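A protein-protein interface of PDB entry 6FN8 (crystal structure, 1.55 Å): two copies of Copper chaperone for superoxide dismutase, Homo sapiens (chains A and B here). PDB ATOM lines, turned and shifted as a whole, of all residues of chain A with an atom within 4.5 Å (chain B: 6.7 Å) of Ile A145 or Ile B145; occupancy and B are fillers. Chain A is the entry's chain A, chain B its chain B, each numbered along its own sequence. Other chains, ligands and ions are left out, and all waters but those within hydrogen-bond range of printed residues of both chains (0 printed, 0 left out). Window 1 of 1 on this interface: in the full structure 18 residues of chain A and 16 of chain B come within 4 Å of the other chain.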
ATOM      1  N   VAL A   6     -30.533  24.422  12.652  1.00  0.00           N
ATOM      2  CA  VAL A   6     -30.038  25.776  12.417  1.00  0.00           C
ATOM      3  C   VAL A   6     -29.510  25.891  10.989  1.00  0.00           C
ATOM      4  O   VAL A   6     -28.877  24.956  10.470  1.00  0.00           O
ATOM      5  CB  VAL A   6     -28.954  26.209  13.433  1.00  0.00           C
ATOM      6  CG1 VAL A   6     -27.681  25.362  13.315  1.00  0.00           C
ATOM      7  CG2 VAL A   6     -28.638  27.689  13.270  1.00  0.00           C
ATOM      8  N   ALA A   7     -29.838  26.999  10.333  1.00  0.00           N
ATOM      9  CA  ALA A   7     -29.227  27.309   9.043  1.00  0.00           C
ATOM     10  C   ALA A   7     -28.402  28.577   9.142  1.00  0.00           C
ATOM     11  O   ALA A   7     -28.922  29.643   9.475  1.00  0.00           O
ATOM     12  CB  ALA A   7     -30.291  27.441   7.961  1.00  0.00           C
ATOM     13  N   ILE A   8     -27.114  28.457   8.838  1.00  0.00           N
ATOM     14  CA  ILE A   8     -26.222  29.610   8.760  1.00  0.00           C
ATOM     15  C   ILE A   8     -26.058  30.009   7.296  1.00  0.00           C
ATOM     16  O   ILE A   8     -25.536  29.232   6.488  1.00  0.00           O
ATOM     17  CB  ILE A   8     -24.844  29.287   9.373  1.00  0.00           C
ATOM     18  CG1 ILE A   8     -25.008  28.837  10.827  1.00  0.00           C
ATOM     19  CG2 ILE A   8     -23.893  30.477   9.258  1.00  0.00           C
ATOM     20  CD1 ILE A   8     -23.723  28.312  11.446  1.00  0.00           C
ATOM     21  N   GLY A  51     -28.954  20.435   0.181  1.00  0.00           N
ATOM     22  CA  GLY A  51     -28.047  21.357   0.864  1.00  0.00           C
ATOM     23  C   GLY A  51     -26.639  21.337   0.295  1.00  0.00           C
ATOM     24  O   GLY A  51     -25.709  21.858   0.897  1.00  0.00           O
ATOM     25  N   LEU A  53     -23.735  22.647  -1.386  1.00  0.00           N
ATOM     26  CA  LEU A  53     -23.233  23.974  -1.716  1.00  0.00           C
ATOM     27  C   LEU A  53     -21.984  23.989  -2.590  1.00  0.00           C
ATOM     28  O   LEU A  53     -21.253  24.989  -2.612  1.00  0.00           O
ATOM     29  CB  LEU A  53     -22.996  24.808  -0.452  1.00  0.00           C
ATOM     30  CG  LEU A  53     -24.170  24.953   0.524  1.00  0.00           C
ATOM     31  CD1 LEU A  53     -23.781  25.850   1.690  1.00  0.00           C
ATOM     32  CD2 LEU A  53     -25.403  25.495  -0.180  1.00  0.00           C
ATOM     33  N   GLY A 111     -30.663  18.699   6.496  1.00  0.00           N
ATOM     34  CA  GLY A 111     -29.747  18.456   5.377  1.00  0.00           C
ATOM     35  C   GLY A 111     -30.190  19.098   4.073  1.00  0.00           C
ATOM     36  O   GLY A 111     -29.501  18.991   3.057  1.00  0.00           O
ATOM     37  N   ARG A 112     -31.318  19.799   4.103  1.00  0.00           N
ATOM     38  CA  ARG A 112     -31.740  20.593   2.944  1.00  0.00           C
ATOM     39  C   ARG A 112     -31.214  22.017   3.098  1.00  0.00           C
ATOM     40  O   ARG A 112     -30.262  22.237   3.830  1.00  0.00           O
ATOM     41  CB  ARG A 112     -33.264  20.540   2.781  1.00  0.00           C
ATOM     42  CG  ARG A 112     -33.767  19.102   2.682  1.00  0.00           C
ATOM     43  CD  ARG A 112     -35.223  19.026   2.248  1.00  0.00           C
ATOM     44  NE  ARG A 112     -35.748  17.664   2.379  1.00  0.00           N
ATOM     45  CZ  ARG A 112     -35.664  16.718   1.446  1.00  0.00           C
ATOM     46  NH1 ARG A 112     -35.031  16.938   0.302  1.00  0.00           N
ATOM     47  NH2 ARG A 112     -36.243  15.538   1.647  1.00  0.00           N
ATOM     48  N   SER A 113     -31.718  22.958   2.306  1.00  0.00           N
ATOM     49  CA  SER A 113     -31.195  24.327   2.380  1.00  0.00           C
ATOM     50  C   SER A 113     -32.305  25.346   2.596  1.00  0.00           C
ATOM     51  O   SER A 113     -33.445  25.144   2.173  1.00  0.00           O
ATOM     52  CB  SER A 113     -30.403  24.696   1.125  1.00  0.00           C
ATOM     53  OG  SER A 113     -31.214  24.501  -0.015  1.00  0.00           O
ATOM     54  N   GLY A 144     -28.163  28.556   3.244  1.00  0.00           N
ATOM     55  CA  GLY A 144     -27.505  27.825   4.328  1.00  0.00           C
ATOM     56  C   GLY A 144     -28.067  26.424   4.440  1.00  0.00           C
ATOM     57  O   GLY A 144     -29.219  26.174   4.079  1.00  0.00           O
ATOM     58  N   ILE A 145     -27.243  25.498   4.912  1.00  0.00           N
ATOM     59  CA  ILE A 145     -27.694  24.138   5.129  1.00  0.00           C
ATOM     60  C   ILE A 145     -28.456  24.032   6.451  1.00  0.00           C
ATOM     61  O   ILE A 145     -28.030  24.577   7.476  1.00  0.00           O
ATOM     62  CB  ILE A 145     -26.496  23.175   5.153  1.00  0.00           C
ATOM     63  CG1 ILE A 145     -25.702  23.310   3.856  1.00  0.00           C
ATOM     64  CG2 ILE A 145     -26.983  21.752   5.362  1.00  0.00           C
ATOM     65  CD1 ILE A 145     -24.301  22.741   3.951  1.00  0.00           C
ATOM     66  N   ILE A 146     -29.591  23.348   6.418  1.00  0.00           N
ATOM     67  CA  ILE A 146     -30.383  23.129   7.629  1.00  0.00           C
ATOM     68  C   ILE A 146     -29.791  21.961   8.415  1.00  0.00           C
ATOM     69  O   ILE A 146     -29.904  20.796   8.020  1.00  0.00           O
ATOM     70  CB  ILE A 146     -31.875  22.915   7.307  1.00  0.00           C
ATOM     71  CG1 ILE A 146     -32.414  24.133   6.537  1.00  0.00           C
ATOM     72  CG2 ILE A 146     -32.685  22.766   8.590  1.00  0.00           C
ATOM     73  CD1 ILE A 146     -33.739  23.870   5.837  1.00  0.00           C
ATOM     74  N   ALA A 147     -29.082  22.297   9.483  1.00  0.00           N
ATOM     75  CA  ALA A 147     -28.234  21.333  10.183  1.00  0.00           C
ATOM     76  C   ALA A 147     -28.881  20.969  11.519  1.00  0.00           C
ATOM     77  O   ALA A 147     -29.491  21.818  12.179  1.00  0.00           O
ATOM     78  CB  ALA A 147     -26.863  21.936  10.425  1.00  0.00           C
ATOM     79  N   VAL B   6     -23.200  15.196   0.829  1.00  0.00           N
ATOM     80  CA  VAL B   6     -21.946  15.876   0.555  1.00  0.00           C
ATOM     81  C   VAL B   6     -21.589  16.774   1.738  1.00  0.00           C
ATOM     82  O   VAL B   6     -22.471  17.371   2.354  1.00  0.00           O
ATOM     83  CB  VAL B   6     -22.017  16.718  -0.746  1.00  0.00           C
ATOM     84  CG1 VAL B   6     -23.100  17.792  -0.643  1.00  0.00           C
ATOM     85  CG2 VAL B   6     -20.665  17.327  -1.076  1.00  0.00           C
ATOM     86  N   ALA B   7     -20.298  16.841   2.058  1.00  0.00           N
ATOM     87  CA  ALA B   7     -19.812  17.752   3.092  1.00  0.00           C
ATOM     88  C   ALA B   7     -18.641  18.561   2.560  1.00  0.00           C
ATOM     89  O   ALA B   7     -17.671  17.998   2.035  1.00  0.00           O
ATOM     90  CB  ALA B   7     -19.399  16.966   4.336  1.00  0.00           C
ATOM     91  N   ILE B   8     -18.685  19.874   2.792  1.00  0.00           N
ATOM     92  CA  ILE B   8     -17.591  20.768   2.457  1.00  0.00           C
ATOM     93  C   ILE B   8     -16.878  21.186   3.741  1.00  0.00           C
ATOM     94  O   ILE B   8     -17.481  21.802   4.617  1.00  0.00           O
ATOM     95  CB  ILE B   8     -18.103  22.010   1.703  1.00  0.00           C
ATOM     96  CG1 ILE B   8     -18.901  21.583   0.468  1.00  0.00           C
ATOM     97  CG2 ILE B   8     -16.957  22.927   1.298  1.00  0.00           C
ATOM     98  CD1 ILE B   8     -19.677  22.732  -0.156  1.00  0.00           C
ATOM     99  N   LEU B   9     -15.632  20.753   3.901  1.00  0.00           N
ATOM    100  CA  LEU B   9     -14.902  21.006   5.146  1.00  0.00           C
ATOM    101  C   LEU B   9     -14.101  22.290   5.097  1.00  0.00           C
ATOM    102  O   LEU B   9     -13.473  22.613   4.078  1.00  0.00           O
ATOM    103  CB  LEU B   9     -13.967  19.840   5.496  1.00  0.00           C
ATOM    104  CG  LEU B   9     -14.645  18.511   5.859  1.00  0.00           C
ATOM    105  CD1 LEU B   9     -15.004  17.751   4.592  1.00  0.00           C
ATOM    106  CD2 LEU B   9     -13.714  17.670   6.728  1.00  0.00           C
ATOM    107  N   GLY B  51     -24.647  19.173  13.080  1.00  0.00           N
ATOM    108  CA  GLY B  51     -24.044  19.961  12.002  1.00  0.00           C
ATOM    109  C   GLY B  51     -24.030  21.452  12.299  1.00  0.00           C
ATOM    110  O   GLY B  51     -23.671  22.272  11.452  1.00  0.00           O
ATOM    111  N   ASP B  52     -24.351  21.782  13.541  1.00  0.00           N
ATOM    112  CA  ASP B  52     -24.438  23.159  14.013  1.00  0.00           C
ATOM    113  C   ASP B  52     -23.045  23.781  14.131  1.00  0.00           C
ATOM    114  O   ASP B  52     -22.219  23.335  14.939  1.00  0.00           O
ATOM    115  CB  ASP B  52     -25.142  23.130  15.375  1.00  0.00           C
ATOM    116  CG  ASP B  52     -25.299  24.504  16.001  1.00  0.00           C
ATOM    117  OD1 ASP B  52     -24.699  25.489  15.516  1.00  0.00           O
ATOM    118  OD2 ASP B  52     -25.992  24.560  17.034  1.00  0.00           O
ATOM    119  N   LEU B  53     -22.761  24.764  13.279  1.00  0.00           N
ATOM    120  CA  LEU B  53     -21.449  25.411  13.243  1.00  0.00           C
ATOM    121  C   LEU B  53     -21.477  26.802  13.879  1.00  0.00           C
ATOM    122  O   LEU B  53     -20.602  27.634  13.608  1.00  0.00           O
ATOM    123  CB  LEU B  53     -20.925  25.518  11.802  1.00  0.00           C
ATOM    124  CG  LEU B  53     -20.596  24.216  11.055  1.00  0.00           C
ATOM    125  CD1 LEU B  53     -19.762  24.471   9.804  1.00  0.00           C
ATOM    126  CD2 LEU B  53     -19.914  23.199  11.958  1.00  0.00           C
ATOM    127  N   VAL B 109     -26.354  10.321   8.266  1.00  0.00           N
ATOM    128  CA  VAL B 109     -25.325  11.368   8.298  1.00  0.00           C
ATOM    129  C   VAL B 109     -25.920  12.750   8.031  1.00  0.00           C
ATOM    130  O   VAL B 109     -25.299  13.766   8.343  1.00  0.00           O
ATOM    131  CB  VAL B 109     -24.135  11.104   7.338  1.00  0.00           C
ATOM    132  CG1 VAL B 109     -23.448   9.786   7.654  1.00  0.00           C
ATOM    133  CG2 VAL B 109     -24.554  11.163   5.877  1.00  0.00           C
ATOM    134  N   GLY B 111     -27.395  16.270   7.824  1.00  0.00           N
ATOM    135  CA  GLY B 111     -27.616  17.255   8.871  1.00  0.00           C
ATOM    136  C   GLY B 111     -26.574  17.204   9.970  1.00  0.00           C
ATOM    137  O   GLY B 111     -26.607  18.013  10.884  1.00  0.00           O
ATOM    138  N   ARG B 112     -25.701  16.201   9.942  1.00  0.00           N
ATOM    139  CA  ARG B 112     -24.667  16.112  10.954  1.00  0.00           C
ATOM    140  C   ARG B 112     -23.372  16.745  10.460  1.00  0.00           C
ATOM    141  O   ARG B 112     -23.403  17.573   9.550  1.00  0.00           O
ATOM    142  CB  ARG B 112     -24.498  14.650  11.386  1.00  0.00           C
ATOM    143  CG  ARG B 112     -25.824  14.041  11.804  1.00  0.00           C
ATOM    144  CD  ARG B 112     -25.661  12.766  12.617  1.00  0.00           C
ATOM    145  NE  ARG B 112     -26.941  12.073  12.762  1.00  0.00           N
ATOM    146  CZ  ARG B 112     -27.755  12.216  13.804  1.00  0.00           C
ATOM    147  NH1 ARG B 112     -27.449  13.050  14.789  1.00  0.00           N
ATOM    148  NH2 ARG B 112     -28.887  11.521  13.850  1.00  0.00           N
ATOM    149  N   SER B 113     -22.252  16.462  11.123  1.00  0.00           N
ATOM    150  CA  SER B 113     -20.968  17.017  10.703  1.00  0.00           C
ATOM    151  C   SER B 113     -19.940  15.928  10.446  1.00  0.00           C
ATOM    152  O   SER B 113     -19.957  14.875  11.086  1.00  0.00           O
ATOM    153  CB  SER B 113     -20.411  17.997  11.742  1.00  0.00           C
ATOM    154  OG  SER B 113     -20.371  17.395  13.030  1.00  0.00           O
ATOM    155  N   LEU B 114     -19.044  16.209   9.510  1.00  0.00           N
ATOM    156  CA  LEU B 114     -17.873  15.386   9.290  1.00  0.00           C
ATOM    157  C   LEU B 114     -16.660  16.181   9.736  1.00  0.00           C
ATOM    158  O   LEU B 114     -16.464  17.329   9.317  1.00  0.00           O
ATOM    159  CB  LEU B 114     -17.753  15.025   7.810  1.00  0.00           C
ATOM    160  CG  LEU B 114     -16.600  14.090   7.455  1.00  0.00           C
ATOM    161  CD1 LEU B 114     -16.809  12.683   8.021  1.00  0.00           C
ATOM    162  CD2 LEU B 114     -16.423  14.069   5.939  1.00  0.00           C
ATOM    163  N   CYS B 143     -14.268  21.031   9.880  1.00  0.00           N
ATOM    164  CA  CYS B 143     -15.551  20.361   9.977  1.00  0.00           C
ATOM    165  C   CYS B 143     -16.417  20.805   8.821  1.00  0.00           C
ATOM    166  O   CYS B 143     -16.249  21.897   8.285  1.00  0.00           O
ATOM    167  CB  CYS B 143     -16.236  20.649  11.320  1.00  0.00           C
ATOM    168  SG  CYS B 143     -16.300  22.401  11.782  1.00  0.00           S
ATOM    169  N   GLY B 144     -17.290  19.915   8.379  1.00  0.00           N
ATOM    170  CA  GLY B 144     -18.193  20.227   7.285  1.00  0.00           C
ATOM    171  C   GLY B 144     -19.578  19.766   7.663  1.00  0.00           C
ATOM    172  O   GLY B 144     -19.742  18.684   8.234  1.00  0.00           O
ATOM    173  N   ILE B 145     -20.586  20.559   7.318  1.00  0.00           N
ATOM    174  CA  ILE B 145     -21.959  20.121   7.446  1.00  0.00           C
ATOM    175  C   ILE B 145     -22.344  19.113   6.363  1.00  0.00           C
ATOM    176  O   ILE B 145     -22.052  19.321   5.180  1.00  0.00           O
ATOM    177  CB  ILE B 145     -22.934  21.312   7.379  1.00  0.00           C
ATOM    178  CG1 ILE B 145     -22.495  22.410   8.351  1.00  0.00           C
ATOM    179  CG2 ILE B 145     -24.351  20.838   7.672  1.00  0.00           C
ATOM    180  CD1 ILE B 145     -23.122  23.757   8.041  1.00  0.00           C
ATOM    181  N   ILE B 146     -22.890  17.974   6.773  1.00  0.00           N
ATOM    182  CA  ILE B 146     -23.261  16.932   5.813  1.00  0.00           C
ATOM    183  C   ILE B 146     -24.672  17.193   5.298  1.00  0.00           C
ATOM    184  O   ILE B 146     -25.631  17.252   6.067  1.00  0.00           O
ATOM    185  CB  ILE B 146     -23.180  15.522   6.426  1.00  0.00           C
ATOM    186  CG1 ILE B 146     -21.790  15.283   7.030  1.00  0.00           C
ATOM    187  CG2 ILE B 146     -23.540  14.455   5.383  1.00  0.00           C
ATOM    188  CD1 ILE B 146     -21.695  13.989   7.823  1.00  0.00           C
ATOM    189  N   ALA B 147     -24.768  17.454   3.997  1.00  0.00           N
ATOM    190  CA  ALA B 147     -26.011  17.911   3.376  1.00  0.00           C
ATOM    191  C   ALA B 147     -26.559  16.841   2.431  1.00  0.00           C
ATOM    192  O   ALA B 147     -25.796  16.070   1.848  1.00  0.00           O
ATOM    193  CB  ALA B 147     -25.745  19.182   2.595  1.00  0.00           C
ATOM    194  N   ARG B 148     -27.873  16.839   2.224  1.00  0.00           N
ATOM    195  CA  ARG B 148     -28.465  16.022   1.167  1.00  0.00           C
ATOM    196  C   ARG B 148     -27.952  16.487  -0.179  1.00  0.00           C
ATOM    197  O   ARG B 148     -27.845  17.687  -0.436  1.00  0.00           O
ATOM    198  CB  ARG B 148     -29.988  16.137   1.162  1.00  0.00           C
ATOM    199  CG  ARG B 148     -30.686  15.691   2.427  1.00  0.00           C
ATOM    200  CD  ARG B 148     -32.191  15.724   2.208  1.00  0.00           C
ATOM    201  NE  ARG B 148     -32.933  15.790   3.459  1.00  0.00           N
ATOM    202  CZ  ARG B 148     -33.697  14.814   3.928  1.00  0.00           C
ATOM    203  NH1 ARG B 148     -34.336  14.981   5.076  1.00  0.00           N
ATOM    204  NH2 ARG B 148     -33.769  13.651   3.286  1.00  0.00           N
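N of Gly B111 is in hydrogen-bond range of O of Ile B146 (2.7 Å). The backbone NH (N) of Ala A147 sits at hydrogen-bond distance from the backbone carbonyl oxygen (O) of Val A6. O of Arg A112 sits at hydrogen-bond distance from N of Ile A146. The backbone NH (N) of Gly B51 is in hydrogen-bond range of the backbone carbonyl oxygen (O) of Gly B111, at 3.2 Å. The backbone carbonyl oxygen (O) of Val B6 sits at hydrogen-bond distance from the backbone NH (N) of Ala B147, 2.8 Å away. The backbone NH (N) of Gly A51 lies within hydrogen-bond range of the backbone carbonyl oxygen (O) of Gly A111, at 3.3 Å.
O of Gly A111 is in hydrogen-bond range of N of Arg B148 (2.8 Å). N of Gly A51 is in hydrogen-bond range of O of Arg B148 (3.0 Å).
Hydrophobic or aromatic side chains of chain A within 4 Å of the printed part of chain B: Val A6, Ile A8, Leu A53, Ile A145 and Ala A147. Hydrophobic or aromatic side chains of chain B within 4 Å of the printed part of chain A: Ile B8, Leu B53, Ile B145 and Ala B147. Among the printed residues, 13 pairs touch across the chains. Among the printed residues, no Asp or Glu carboxylate lies within 4 Å of a Lys or Arg side-chain nitrogen of the other chain.
Ile A8 touches Leu B53, and with the chains exchanged Leu A53 touches Ile B8. Gly A51 touches Ala B147, and with the chains exchanged Ala A147 touches Gly B51. Gly A111 touches Ala B147, and with the chains exchanged Ala A147 touches Gly B111. Ile A145 touches Ala B147, and with the chains exchanged Ala A147 touches Ile B145. Positions printed for both chains: 6, 7, 8, 51, 53, 111, 112, 113, 144, 145, 146 and 147. Of the 13 pairs that touch across the chains among the printed residues, 9 have their exchanged pair printed and touching as well.
Ile A145 touches two residues of chain B. Of chain A, only Ile A145 (3.6 Å) and Ala A147 (3.9 Å) come within 4 Å of Ile B145. Of the printed residues of chain A, Gly B51 touches Ala A147. Of the printed residues of chain B, Val A6 touches Asp B52. Gly A144 touches none of the printed residues of chain B. Ala B7 touches none of the printed residues of chain A. The nearest printed residue of chain A that does not touch Ile B145 is Ile A146 (5.6 Å).
Leu B53 touches Ile A8 (C to CD1, 3.6 Å). Gly A51 touches Ala B147. C of Leu A53 touches CD1 of Ile B8 (3.6 Å). CA of Ala B147 touches O of Gly A111, at 3.7 Å. Arg B148 touches Arg A112. Ile B145 touches Ile A145 (CG2 to CG2, 3.6 Å). Ala B147 touches Ile A145. Ala A147 touches Gly B51. Gly B111 touches Ala A147 (O to CA, 3.8 Å). Ala A147 touches Ile B145 (CB to CG2, 3.9 Å).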
